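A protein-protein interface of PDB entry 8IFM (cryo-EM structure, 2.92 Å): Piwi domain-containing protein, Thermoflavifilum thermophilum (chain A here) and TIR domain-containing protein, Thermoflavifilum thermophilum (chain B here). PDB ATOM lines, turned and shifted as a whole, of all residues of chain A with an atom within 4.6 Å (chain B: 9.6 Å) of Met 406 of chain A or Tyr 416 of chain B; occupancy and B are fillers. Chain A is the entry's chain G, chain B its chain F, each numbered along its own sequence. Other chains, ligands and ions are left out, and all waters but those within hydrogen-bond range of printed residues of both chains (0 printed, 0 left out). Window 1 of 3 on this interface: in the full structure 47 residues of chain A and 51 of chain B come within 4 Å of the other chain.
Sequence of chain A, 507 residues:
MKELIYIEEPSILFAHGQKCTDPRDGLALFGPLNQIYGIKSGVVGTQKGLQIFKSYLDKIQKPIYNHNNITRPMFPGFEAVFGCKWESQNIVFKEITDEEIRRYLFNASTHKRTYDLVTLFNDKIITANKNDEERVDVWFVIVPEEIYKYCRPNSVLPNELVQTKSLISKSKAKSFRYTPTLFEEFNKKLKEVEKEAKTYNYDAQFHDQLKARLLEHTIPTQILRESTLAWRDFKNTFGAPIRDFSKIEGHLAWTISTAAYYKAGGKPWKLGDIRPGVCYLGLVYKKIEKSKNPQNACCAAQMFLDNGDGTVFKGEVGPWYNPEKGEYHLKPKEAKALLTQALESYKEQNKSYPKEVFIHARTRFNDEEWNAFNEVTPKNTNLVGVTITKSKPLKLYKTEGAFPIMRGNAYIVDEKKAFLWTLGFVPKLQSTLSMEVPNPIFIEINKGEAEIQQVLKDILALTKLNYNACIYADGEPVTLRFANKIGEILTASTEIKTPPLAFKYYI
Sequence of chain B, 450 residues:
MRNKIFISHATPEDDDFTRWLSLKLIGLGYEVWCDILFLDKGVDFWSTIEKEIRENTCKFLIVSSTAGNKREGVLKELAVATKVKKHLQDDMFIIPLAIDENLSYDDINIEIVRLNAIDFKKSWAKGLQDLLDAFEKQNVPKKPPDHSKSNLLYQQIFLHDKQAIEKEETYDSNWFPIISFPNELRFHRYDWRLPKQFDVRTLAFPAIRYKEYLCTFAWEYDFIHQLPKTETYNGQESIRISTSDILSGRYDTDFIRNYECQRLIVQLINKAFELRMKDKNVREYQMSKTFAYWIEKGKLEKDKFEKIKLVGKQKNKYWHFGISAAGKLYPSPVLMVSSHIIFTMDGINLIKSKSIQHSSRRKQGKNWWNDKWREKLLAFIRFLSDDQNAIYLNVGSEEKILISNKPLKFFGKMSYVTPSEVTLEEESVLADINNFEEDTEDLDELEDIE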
ATOM      1  N   TYR A   6     -13.026  15.728  23.169  1.00  0.00           N
ATOM      2  CA  TYR A   6     -13.469  14.806  24.205  1.00  0.00           C
ATOM      3  C   TYR A   6     -14.987  14.768  24.262  1.00  0.00           C
ATOM      4  O   TYR A   6     -15.642  15.816  24.254  1.00  0.00           O
ATOM      5  CB  TYR A   6     -12.905  15.190  25.574  1.00  0.00           C
ATOM      6  CG  TYR A   6     -13.100  14.110  26.613  1.00  0.00           C
ATOM      7  CD1 TYR A   6     -12.542  12.851  26.456  1.00  0.00           C
ATOM      8  CD2 TYR A   6     -13.852  14.354  27.755  1.00  0.00           C
ATOM      9  CE1 TYR A   6     -12.736  11.864  27.402  1.00  0.00           C
ATOM     10  CE2 TYR A   6     -14.043  13.374  28.708  1.00  0.00           C
ATOM     11  CZ  TYR A   6     -13.480  12.131  28.527  1.00  0.00           C
ATOM     12  OH  TYR A   6     -13.664  11.147  29.471  1.00  0.00           O
ATOM     13  N   LYS A 398       0.606   7.442  22.283  1.00  0.00           N
ATOM     14  CA  LYS A 398       0.867   8.505  23.250  1.00  0.00           C
ATOM     15  C   LYS A 398       2.373   8.569  23.456  1.00  0.00           C
ATOM     16  O   LYS A 398       2.967   7.629  23.992  1.00  0.00           O
ATOM     17  CB  LYS A 398       0.147   8.242  24.573  1.00  0.00           C
ATOM     18  CG  LYS A 398      -0.716   9.390  25.051  1.00  0.00           C
ATOM     19  CD  LYS A 398      -1.434   9.043  26.343  1.00  0.00           C
ATOM     20  CE  LYS A 398      -0.646   9.521  27.548  1.00  0.00           C
ATOM     21  NZ  LYS A 398      -1.531   9.973  28.655  1.00  0.00           N
ATOM     22  N   PHE A 403       0.999   4.255  28.604  1.00  0.00           N
ATOM     23  CA  PHE A 403      -0.332   3.692  28.495  1.00  0.00           C
ATOM     24  C   PHE A 403      -1.049   4.282  27.284  1.00  0.00           C
ATOM     25  O   PHE A 403      -0.747   5.403  26.865  1.00  0.00           O
ATOM     26  CB  PHE A 403      -1.147   3.965  29.767  1.00  0.00           C
ATOM     27  CG  PHE A 403      -0.754   3.107  30.937  1.00  0.00           C
ATOM     28  CD1 PHE A 403       0.490   3.246  31.527  1.00  0.00           C
ATOM     29  CD2 PHE A 403      -1.629   2.165  31.448  1.00  0.00           C
ATOM     30  CE1 PHE A 403       0.855   2.459  32.600  1.00  0.00           C
ATOM     31  CE2 PHE A 403      -1.270   1.378  32.524  1.00  0.00           C
ATOM     32  CZ  PHE A 403      -0.027   1.525  33.100  1.00  0.00           C
ATOM     33  N   PRO A 404      -1.997   3.548  26.699  1.00  0.00           N
ATOM     34  CA  PRO A 404      -2.634   4.009  25.459  1.00  0.00           C
ATOM     35  C   PRO A 404      -3.469   5.269  25.609  1.00  0.00           C
ATOM     36  O   PRO A 404      -3.644   5.793  26.712  1.00  0.00           O
ATOM     37  CB  PRO A 404      -3.509   2.814  25.062  1.00  0.00           C
ATOM     38  CG  PRO A 404      -2.847   1.647  25.691  1.00  0.00           C
ATOM     39  CD  PRO A 404      -2.373   2.162  27.011  1.00  0.00           C
ATOM     40  N   ILE A 405      -3.980   5.761  24.478  1.00  0.00           N
ATOM     41  CA  ILE A 405      -4.828   6.944  24.486  1.00  0.00           C
ATOM     42  C   ILE A 405      -6.079   6.672  25.306  1.00  0.00           C
ATOM     43  O   ILE A 405      -6.717   5.621  25.174  1.00  0.00           O
ATOM     44  CB  ILE A 405      -5.178   7.359  23.050  1.00  0.00           C
ATOM     45  CG1 ILE A 405      -6.321   8.378  23.053  1.00  0.00           C
ATOM     46  CG2 ILE A 405      -5.526   6.142  22.211  1.00  0.00           C
ATOM     47  CD1 ILE A 405      -6.341   9.281  21.854  1.00  0.00           C
ATOM     48  N   MET A 406      -6.427   7.623  26.168  1.00  0.00           N
ATOM     49  CA  MET A 406      -7.607   7.483  27.007  1.00  0.00           C
ATOM     50  C   MET A 406      -8.878   7.417  26.170  1.00  0.00           C
ATOM     51  O   MET A 406      -9.039   8.145  25.187  1.00  0.00           O
ATOM     52  CB  MET A 406      -7.660   8.638  28.007  1.00  0.00           C
ATOM     53  CG  MET A 406      -9.004   8.906  28.632  1.00  0.00           C
ATOM     54  SD  MET A 406      -9.145  10.684  28.865  1.00  0.00           S
ATOM     55  CE  MET A 406      -9.510  11.199  27.194  1.00  0.00           C
ATOM     56  N   ARG A 407      -9.777   6.518  26.568  1.00  0.00           N
ATOM     57  CA  ARG A 407     -11.023   6.302  25.845  1.00  0.00           C
ATOM     58  C   ARG A 407     -11.879   7.561  25.846  1.00  0.00           C
ATOM     59  O   ARG A 407     -11.900   8.320  26.819  1.00  0.00           O
ATOM     60  CB  ARG A 407     -11.787   5.135  26.475  1.00  0.00           C
ATOM     61  CG  ARG A 407     -13.078   4.761  25.772  1.00  0.00           C
ATOM     62  CD  ARG A 407     -14.194   4.482  26.766  1.00  0.00           C
ATOM     63  NE  ARG A 407     -15.305   3.767  26.150  1.00  0.00           N
ATOM     64  CZ  ARG A 407     -16.537   4.246  26.051  1.00  0.00           C
ATOM     65  NH1 ARG A 407     -16.860   5.430  26.540  1.00  0.00           N
ATOM     66  NH2 ARG A 407     -17.470   3.516  25.444  1.00  0.00           N
ATOM     67  N   GLY A 408     -12.592   7.780  24.744  1.00  0.00           N
ATOM     68  CA  GLY A 408     -13.442   8.937  24.582  1.00  0.00           C
ATOM     69  C   GLY A 408     -12.877  10.023  23.691  1.00  0.00           C
ATOM     70  O   GLY A 408     -13.619  10.938  23.313  1.00  0.00           O
ATOM     71  N   ASN A 409     -11.595   9.951  23.347  1.00  0.00           N
ATOM     72  CA  ASN A 409     -10.991  10.929  22.454  1.00  0.00           C
ATOM     73  C   ASN A 409     -11.443  10.686  21.021  1.00  0.00           C
ATOM     74  O   ASN A 409     -11.549   9.540  20.574  1.00  0.00           O
ATOM     75  CB  ASN A 409      -9.468  10.862  22.544  1.00  0.00           C
ATOM     76  CG  ASN A 409      -8.914  11.724  23.659  1.00  0.00           C
ATOM     77  OD1 ASN A 409      -9.601  12.603  24.178  1.00  0.00           O
ATOM     78  ND2 ASN A 409      -7.665  11.477  24.034  1.00  0.00           N
ATOM     79  N   PHE A 425      -7.636   3.025  27.185  1.00  0.00           N
ATOM     80  CA  PHE A 425      -7.401   3.292  28.597  1.00  0.00           C
ATOM     81  C   PHE A 425      -8.535   4.136  29.163  1.00  0.00           C
ATOM     82  O   PHE A 425      -8.990   5.097  28.540  1.00  0.00           O
ATOM     83  CB  PHE A 425      -6.049   3.993  28.788  1.00  0.00           C
ATOM     84  CG  PHE A 425      -5.700   4.283  30.232  1.00  0.00           C
ATOM     85  CD1 PHE A 425      -6.318   5.310  30.930  1.00  0.00           C
ATOM     86  CD2 PHE A 425      -4.754   3.517  30.890  1.00  0.00           C
ATOM     87  CE1 PHE A 425      -5.999   5.565  32.248  1.00  0.00           C
ATOM     88  CE2 PHE A 425      -4.433   3.772  32.210  1.00  0.00           C
ATOM     89  CZ  PHE A 425      -5.055   4.797  32.886  1.00  0.00           C
ATOM     90  N   PRO A 427      -9.379   6.169  32.839  1.00  0.00           N
ATOM     91  CA  PRO A 427      -8.886   6.507  34.183  1.00  0.00           C
ATOM     92  C   PRO A 427      -9.649   5.808  35.291  1.00  0.00           C
ATOM     93  O   PRO A 427      -9.042   5.392  36.286  1.00  0.00           O
ATOM     94  CB  PRO A 427      -9.055   8.033  34.244  1.00  0.00           C
ATOM     95  CG  PRO A 427      -9.213   8.471  32.823  1.00  0.00           C
ATOM     96  CD  PRO A 427      -9.898   7.348  32.128  1.00  0.00           C
ATOM     97  N   ASP B 161      -9.413   9.589  42.794  1.00  0.00           N
ATOM     98  CA  ASP B 161      -7.995   9.296  42.609  1.00  0.00           C
ATOM     99  C   ASP B 161      -7.640   9.086  41.145  1.00  0.00           C
ATOM    100  O   ASP B 161      -6.470   9.222  40.771  1.00  0.00           O
ATOM    101  CB  ASP B 161      -7.600   8.060  43.420  1.00  0.00           C
ATOM    102  CG  ASP B 161      -7.045   8.411  44.783  1.00  0.00           C
ATOM    103  OD1 ASP B 161      -6.492   9.521  44.934  1.00  0.00           O
ATOM    104  OD2 ASP B 161      -7.161   7.579  45.706  1.00  0.00           O
ATOM    105  N   LYS B 162      -8.625   8.757  40.314  1.00  0.00           N
ATOM    106  CA  LYS B 162      -8.410   8.523  38.892  1.00  0.00           C
ATOM    107  C   LYS B 162      -9.663   8.883  38.104  1.00  0.00           C
ATOM    108  O   LYS B 162     -10.745   8.344  38.349  1.00  0.00           O
ATOM    109  CB  LYS B 162      -7.942   7.077  38.663  1.00  0.00           C
ATOM    110  CG  LYS B 162      -8.596   5.970  39.522  1.00  0.00           C
ATOM    111  CD  LYS B 162     -10.076   5.723  39.348  1.00  0.00           C
ATOM    112  CE  LYS B 162     -10.586   4.796  40.442  1.00  0.00           C
ATOM    113  NZ  LYS B 162     -12.069   4.701  40.463  1.00  0.00           N
ATOM    114  N   GLN B 163      -9.516   9.824  37.178  1.00  0.00           N
ATOM    115  CA  GLN B 163     -10.647  10.417  36.471  1.00  0.00           C
ATOM    116  C   GLN B 163     -10.097  11.163  35.259  1.00  0.00           C
ATOM    117  O   GLN B 163      -8.888  11.174  35.007  1.00  0.00           O
ATOM    118  CB  GLN B 163     -11.444  11.341  37.395  1.00  0.00           C
ATOM    119  CG  GLN B 163     -12.915  11.490  37.046  1.00  0.00           C
ATOM    120  CD  GLN B 163     -13.668  12.332  38.058  1.00  0.00           C
ATOM    121  OE1 GLN B 163     -14.492  11.823  38.815  1.00  0.00           O
ATOM    122  NE2 GLN B 163     -13.384  13.629  38.075  1.00  0.00           N
ATOM    123  N   ALA B 164     -10.998  11.793  34.510  1.00  0.00           N
ATOM    124  CA  ALA B 164     -10.623  12.597  33.354  1.00  0.00           C
ATOM    125  C   ALA B 164     -10.286  14.009  33.819  1.00  0.00           C
ATOM    126  O   ALA B 164     -11.100  14.657  34.487  1.00  0.00           O
ATOM    127  CB  ALA B 164     -11.750  12.622  32.324  1.00  0.00           C
ATOM    128  N   ILE B 165      -9.093  14.481  33.467  1.00  0.00           N
ATOM    129  CA  ILE B 165      -8.611  15.784  33.902  1.00  0.00           C
ATOM    130  C   ILE B 165      -8.393  16.668  32.683  1.00  0.00           C
ATOM    131  O   ILE B 165      -8.148  16.186  31.573  1.00  0.00           O
ATOM    132  CB  ILE B 165      -7.311  15.673  34.727  1.00  0.00           C
ATOM    133  CG1 ILE B 165      -6.364  14.658  34.089  1.00  0.00           C
ATOM    134  CG2 ILE B 165      -7.623  15.290  36.163  1.00  0.00           C
ATOM    135  CD1 ILE B 165      -5.011  14.590  34.750  1.00  0.00           C
ATOM    136  N   GLU B 166      -8.483  17.982  32.902  1.00  0.00           N
ATOM    137  CA  GLU B 166      -8.269  18.975  31.850  1.00  0.00           C
ATOM    138  C   GLU B 166      -6.764  19.143  31.632  1.00  0.00           C
ATOM    139  O   GLU B 166      -6.156  20.170  31.940  1.00  0.00           O
ATOM    140  CB  GLU B 166      -8.945  20.288  32.225  1.00  0.00           C
ATOM    141  CG  GLU B 166      -8.964  21.355  31.136  1.00  0.00           C
ATOM    142  CD  GLU B 166      -9.348  20.810  29.776  1.00  0.00           C
ATOM    143  OE1 GLU B 166     -10.387  20.123  29.677  1.00  0.00           O
ATOM    144  OE2 GLU B 166      -8.617  21.080  28.802  1.00  0.00           O
ATOM    145  N   LYS B 167      -6.158  18.090  31.088  1.00  0.00           N
ATOM    146  CA  LYS B 167      -4.717  18.021  30.883  1.00  0.00           C
ATOM    147  C   LYS B 167      -4.417  17.874  29.399  1.00  0.00           C
ATOM    148  O   LYS B 167      -5.018  17.034  28.721  1.00  0.00           O
ATOM    149  CB  LYS B 167      -4.108  16.852  31.663  1.00  0.00           C
ATOM    150  CG  LYS B 167      -2.847  16.280  31.037  1.00  0.00           C
ATOM    151  CD  LYS B 167      -2.197  15.238  31.931  1.00  0.00           C
ATOM    152  CE  LYS B 167      -1.063  14.526  31.211  1.00  0.00           C
ATOM    153  NZ  LYS B 167      -0.303  13.620  32.116  1.00  0.00           N
ATOM    154  N   GLU B 168      -3.488  18.686  28.900  1.00  0.00           N
ATOM    155  CA  GLU B 168      -3.093  18.619  27.501  1.00  0.00           C
ATOM    156  C   GLU B 168      -2.173  17.424  27.299  1.00  0.00           C
ATOM    157  O   GLU B 168      -1.255  17.192  28.094  1.00  0.00           O
ATOM    158  CB  GLU B 168      -2.428  19.940  27.083  1.00  0.00           C
ATOM    159  CG  GLU B 168      -2.085  20.148  25.586  1.00  0.00           C
ATOM    160  CD  GLU B 168      -0.935  19.308  25.028  1.00  0.00           C
ATOM    161  OE1 GLU B 168      -0.268  18.566  25.774  1.00  0.00           O
ATOM    162  OE2 GLU B 168      -0.693  19.405  23.807  1.00  0.00           O
ATOM    163  N   GLU B 169      -2.426  16.659  26.240  1.00  0.00           N
ATOM    164  CA  GLU B 169      -1.622  15.496  25.901  1.00  0.00           C
ATOM    165  C   GLU B 169      -1.340  15.506  24.406  1.00  0.00           C
ATOM    166  O   GLU B 169      -2.132  16.029  23.618  1.00  0.00           O
ATOM    167  CB  GLU B 169      -2.330  14.193  26.293  1.00  0.00           C
ATOM    168  CG  GLU B 169      -1.552  13.324  27.269  1.00  0.00           C
ATOM    169  CD  GLU B 169      -0.223  12.849  26.725  1.00  0.00           C
ATOM    170  OE1 GLU B 169      -0.062  12.802  25.490  1.00  0.00           O
ATOM    171  OE2 GLU B 169       0.662  12.521  27.541  1.00  0.00           O
ATOM    172  N   THR B 170      -0.208  14.923  24.018  1.00  0.00           N
ATOM    173  CA  THR B 170       0.214  14.888  22.624  1.00  0.00           C
ATOM    174  C   THR B 170       0.436  13.447  22.178  1.00  0.00           C
ATOM    175  O   THR B 170       0.880  12.599  22.959  1.00  0.00           O
ATOM    176  CB  THR B 170       1.474  15.746  22.407  1.00  0.00           C
ATOM    177  OG1 THR B 170       1.566  16.129  21.028  1.00  0.00           O
ATOM    178  CG2 THR B 170       2.732  15.014  22.825  1.00  0.00           C
ATOM    179  N   TYR B 171       0.102  13.176  20.917  1.00  0.00           N
ATOM    180  CA  TYR B 171      -0.042  11.824  20.398  1.00  0.00           C
ATOM    181  C   TYR B 171       0.675  11.670  19.065  1.00  0.00           C
ATOM    182  O   TYR B 171       0.554  12.525  18.181  1.00  0.00           O
ATOM    183  CB  TYR B 171      -1.517  11.474  20.188  1.00  0.00           C
ATOM    184  CG  TYR B 171      -2.418  11.726  21.368  1.00  0.00           C
ATOM    185  CD1 TYR B 171      -2.503  10.813  22.408  1.00  0.00           C
ATOM    186  CD2 TYR B 171      -3.201  12.868  21.435  1.00  0.00           C
ATOM    187  CE1 TYR B 171      -3.335  11.036  23.485  1.00  0.00           C
ATOM    188  CE2 TYR B 171      -4.034  13.101  22.508  1.00  0.00           C
ATOM    189  CZ  TYR B 171      -4.097  12.181  23.530  1.00  0.00           C
ATOM    190  OH  TYR B 171      -4.927  12.406  24.605  1.00  0.00           O
ATOM    191  N   TRP B 369       2.774  -2.479  24.904  1.00  0.00           N
ATOM    192  CA  TRP B 369       1.745  -1.471  25.131  1.00  0.00           C
ATOM    193  C   TRP B 369       2.117  -0.230  24.325  1.00  0.00           C
ATOM    194  O   TRP B 369       2.964  -0.278  23.429  1.00  0.00           O
ATOM    195  CB  TRP B 369       1.570  -1.207  26.634  1.00  0.00           C
ATOM    196  CG  TRP B 369       1.304  -2.459  27.410  1.00  0.00           C
ATOM    197  CD1 TRP B 369       2.209  -3.194  28.116  1.00  0.00           C
ATOM    198  CD2 TRP B 369       0.049  -3.137  27.540  1.00  0.00           C
ATOM    199  NE1 TRP B 369       1.594  -4.283  28.684  1.00  0.00           N
ATOM    200  CE2 TRP B 369       0.267  -4.270  28.345  1.00  0.00           C
ATOM    201  CE3 TRP B 369      -1.240  -2.891  27.056  1.00  0.00           C
ATOM    202  CZ2 TRP B 369      -0.756  -5.156  28.678  1.00  0.00           C
ATOM    203  CZ3 TRP B 369      -2.251  -3.771  27.386  1.00  0.00           C
ATOM    204  CH2 TRP B 369      -2.004  -4.890  28.189  1.00  0.00           C
ATOM    205  N   ASN B 370       1.463   0.889  24.643  1.00  0.00           N
ATOM    206  CA  ASN B 370       1.548   2.090  23.814  1.00  0.00           C
ATOM    207  C   ASN B 370       2.993   2.522  23.592  1.00  0.00           C
ATOM    208  O   ASN B 370       3.406   2.785  22.456  1.00  0.00           O
ATOM    209  CB  ASN B 370       0.726   3.207  24.466  1.00  0.00           C
ATOM    210  CG  ASN B 370       0.784   4.525  23.707  1.00  0.00           C
ATOM    211  OD1 ASN B 370       1.846   5.001  23.307  1.00  0.00           O
ATOM    212  ND2 ASN B 370      -0.383   5.115  23.492  1.00  0.00           N
ATOM    213  N   ASP B 371       3.777   2.603  24.669  1.00  0.00           N
ATOM    214  CA  ASP B 371       5.145   3.097  24.546  1.00  0.00           C
ATOM    215  C   ASP B 371       5.971   2.202  23.629  1.00  0.00           C
ATOM    216  O   ASP B 371       6.682   2.690  22.744  1.00  0.00           O
ATOM    217  CB  ASP B 371       5.779   3.241  25.937  1.00  0.00           C
ATOM    218  CG  ASP B 371       6.142   1.905  26.585  1.00  0.00           C
ATOM    219  OD1 ASP B 371       6.914   1.116  26.002  1.00  0.00           O
ATOM    220  OD2 ASP B 371       5.645   1.640  27.699  1.00  0.00           O
ATOM    221  N   GLY B 412      -4.743  16.600  22.545  1.00  0.00           N
ATOM    222  CA  GLY B 412      -6.052  16.664  23.161  1.00  0.00           C
ATOM    223  C   GLY B 412      -6.013  17.440  24.460  1.00  0.00           C
ATOM    224  O   GLY B 412      -5.008  17.458  25.172  1.00  0.00           O
ATOM    225  N   LYS B 413      -7.139  18.089  24.762  1.00  0.00           N
ATOM    226  CA  LYS B 413      -7.247  18.909  25.961  1.00  0.00           C
ATOM    227  C   LYS B 413      -7.566  18.098  27.211  1.00  0.00           C
ATOM    228  O   LYS B 413      -7.414  18.614  28.323  1.00  0.00           O
ATOM    229  CB  LYS B 413      -8.317  19.986  25.761  1.00  0.00           C
ATOM    230  CG  LYS B 413      -7.975  21.000  24.680  1.00  0.00           C
ATOM    231  CD  LYS B 413      -8.365  22.407  25.093  1.00  0.00           C
ATOM    232  CE  LYS B 413      -8.402  23.341  23.892  1.00  0.00           C
ATOM    233  NZ  LYS B 413      -8.516  24.770  24.296  1.00  0.00           N
ATOM    234  N   MET B 414      -7.996  16.848  27.060  1.00  0.00           N
ATOM    235  CA  MET B 414      -8.337  15.986  28.183  1.00  0.00           C
ATOM    236  C   MET B 414      -7.474  14.732  28.146  1.00  0.00           C
ATOM    237  O   MET B 414      -7.224  14.171  27.076  1.00  0.00           O
ATOM    238  CB  MET B 414      -9.819  15.600  28.159  1.00  0.00           C
ATOM    239  CG  MET B 414     -10.752  16.675  28.688  1.00  0.00           C
ATOM    240  SD  MET B 414     -11.153  16.441  30.430  1.00  0.00           S
ATOM    241  CE  MET B 414     -12.421  17.684  30.657  1.00  0.00           C
ATOM    242  N   SER B 415      -7.020  14.300  29.317  1.00  0.00           N
ATOM    243  CA  SER B 415      -6.145  13.139  29.410  1.00  0.00           C
ATOM    244  C   SER B 415      -6.246  12.559  30.819  1.00  0.00           C
ATOM    245  O   SER B 415      -7.173  12.881  31.571  1.00  0.00           O
ATOM    246  CB  SER B 415      -4.704  13.517  29.033  1.00  0.00           C
ATOM    247  OG  SER B 415      -3.835  12.415  29.222  1.00  0.00           O
ATOM    248  N   TYR B 416      -5.294  11.698  31.170  1.00  0.00           N
ATOM    249  CA  TYR B 416      -5.279  10.995  32.442  1.00  0.00           C
ATOM    250  C   TYR B 416      -3.889  11.075  33.055  1.00  0.00           C
ATOM    251  O   TYR B 416      -2.899  11.340  32.370  1.00  0.00           O
ATOM    252  CB  TYR B 416      -5.675   9.524  32.270  1.00  0.00           C
ATOM    253  CG  TYR B 416      -4.757   8.765  31.336  1.00  0.00           C
ATOM    254  CD1 TYR B 416      -4.972   8.778  29.969  1.00  0.00           C
ATOM    255  CD2 TYR B 416      -3.673   8.046  31.820  1.00  0.00           C
ATOM    256  CE1 TYR B 416      -4.144   8.096  29.107  1.00  0.00           C
ATOM    257  CE2 TYR B 416      -2.835   7.360  30.963  1.00  0.00           C
ATOM    258  CZ  TYR B 416      -3.078   7.389  29.608  1.00  0.00           C
ATOM    259  OH  TYR B 416      -2.254   6.714  28.742  1.00  0.00           O
ATOM    260  N   VAL B 417      -3.827  10.842  34.361  1.00  0.00           N
ATOM    261  CA  VAL B 417      -2.549  10.673  35.043  1.00  0.00           C
ATOM    262  C   VAL B 417      -2.052   9.253  34.806  1.00  0.00           C
ATOM    263  O   VAL B 417      -2.778   8.279  35.035  1.00  0.00           O
ATOM    264  CB  VAL B 417      -2.683  10.985  36.543  1.00  0.00           C
ATOM    265  CG1 VAL B 417      -2.844  12.478  36.756  1.00  0.00           C
ATOM    266  CG2 VAL B 417      -3.870  10.248  37.142  1.00  0.00           C
ATOM    267  N   THR B 418      -0.824   9.132  34.327  1.00  0.00           N
ATOM    268  CA  THR B 418      -0.287   7.823  33.975  1.00  0.00           C
ATOM    269  C   THR B 418       0.087   7.040  35.228  1.00  0.00           C
ATOM    270  O   THR B 418       0.910   7.514  36.023  1.00  0.00           O
ATOM    271  CB  THR B 418       0.920   7.976  33.050  1.00  0.00           C
ATOM    272  OG1 THR B 418       1.638   6.736  32.980  1.00  0.00           O
ATOM    273  CG2 THR B 418       1.847   9.088  33.532  1.00  0.00           C
ATOM    274  N   PRO B 419      -0.492   5.861  35.455  1.00  0.00           N
ATOM    275  CA  PRO B 419      -0.129   5.074  36.640  1.00  0.00           C
ATOM    276  C   PRO B 419       1.100   4.212  36.408  1.00  0.00           C
ATOM    277  O   PRO B 419       1.076   3.311  35.565  1.00  0.00           O
ATOM    278  CB  PRO B 419      -1.378   4.210  36.883  1.00  0.00           C
ATOM    279  CG  PRO B 419      -2.415   4.683  35.863  1.00  0.00           C
ATOM    280  CD  PRO B 419      -1.627   5.260  34.741  1.00  0.00           C
ATOM    281  N   SER B 420       2.171   4.466  37.152  1.00  0.00           N
ATOM    282  CA  SER B 420       3.391   3.675  37.022  1.00  0.00           C
ATOM    283  C   SER B 420       4.280   3.828  38.250  1.00  0.00           C
ATOM    284  O   SER B 420       5.423   3.369  38.260  1.00  0.00           O
ATOM    285  CB  SER B 420       4.163   4.077  35.764  1.00  0.00           C
ATOM    286  OG  SER B 420       5.558   3.913  35.949  1.00  0.00           O
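ND2 of Asn 370 of chain B is in hydrogen-bond range of O of Phe 403 of chain A. O of Phe 403 of chain A is in hydrogen-bond range of OH of Tyr 416 of chain B, at 2.7 Å. OH of Tyr 416 of chain B lies within hydrogen-bond range of O of Pro 404 of chain A. The side-chain hydroxyl (OG) of Ser 415 of chain B is in hydrogen-bond range of the side-chain amino group (NZ) of Lys 398 of chain A, 3.4 Å away. The side-chain amino group (NZ) of Lys 398 of chain A lies within salt-bridge range of the side-chain carboxylate (OE2) of Glu 169 of chain B (3.5 Å). ND2 of Asn 370 of chain B sits close to N of Lys 398 of chain A (2.8 Å). The side-chain hydroxyl of Tyr 416 of chain B sits close to the side-chain amino group of Lys 398 of chain A, at 3.3 Å. OH of Tyr 171 of chain B lies within hydrogen-bond range of ND2 of Asn 409 of chain A.
N of Met 414 of chain B lies close to O of Lys 167 of chain B (3.4 Å). The backbone carbonyl oxygen (O) of Glu 169 of chain B lies within hydrogen-bond range of the backbone NH (N) of Gly 412 of chain B (2.9 Å).
Printed residues of chain B that touch a printed residue of chain A: Lys 162, Gln 163, Ala 164, Glu 169, Tyr 171, Asn 370, Met 414, Ser 415, Tyr 416, Thr 418 and Pro 419. Hydrophobic or aromatic side chains of chain B that line the printed part of chain A: Ala 164, Tyr 171, Met 414, Tyr 416 and Pro 419. Among the printed residues, 24 pairs touch across the chains. Among the printed residues, Asp or Glu carboxylates within 4 Å of a Lys or Arg side-chain nitrogen of the other chain: Lys 398 of chain A with Glu 169 of chain B (3.5 Å).
Among the printed residues, merely in contact across the chains: Phe 403 of chain A with Pro 419 of chain B, Pro 427 of chain A with Lys 162 of chain B, Pro 404 of chain A with Asn 370 of chain B, Pro 427 of chain A with Gln 163 of chain B, Met 406 of chain A with Tyr 416 of chain B, Phe 425 of chain A with Tyr 416 of chain B, Lys 398 of chain A with Tyr 171 of chain B, Pro 427 of chain A with Tyr 416 of chain B, Tyr 6 of chain A with Ala 164 of chain B, Met 406 of chain A with Met 414 of chain B, Ile 405 of chain A with Asn 370 of chain B, Ile 405 of chain A with Tyr 171 of chain B, Met 406 of chain A with Ser 415 of chain B, Tyr 6 of chain A with Met 414 of chain B, Phe 425 of chain A with Pro 419 of chain B and Phe 403 of chain A with Thr 418 of chain B.
Of chain B, only Tyr 171 (3.8 Å) and Asn 370 (3.8 Å) come within 4 Å of Ile 405 of chain A. Asn 409 of chain A touches one residue of chain B. Printed residues of chain B within 4 Å of Phe 425 of chain A: Tyr 416 (3.4 Å) and Pro 419 (3.9 Å). Printed residues of chain A within 4 Å of Gln 163 of chain B: Pro 427 (3.2 Å). Thr 170 of chain B touches none of the printed residues of chain A. The nearest residue of chain B that does not touch Met 406 of chain A is Ala 164 of chain B (4.7 Å).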
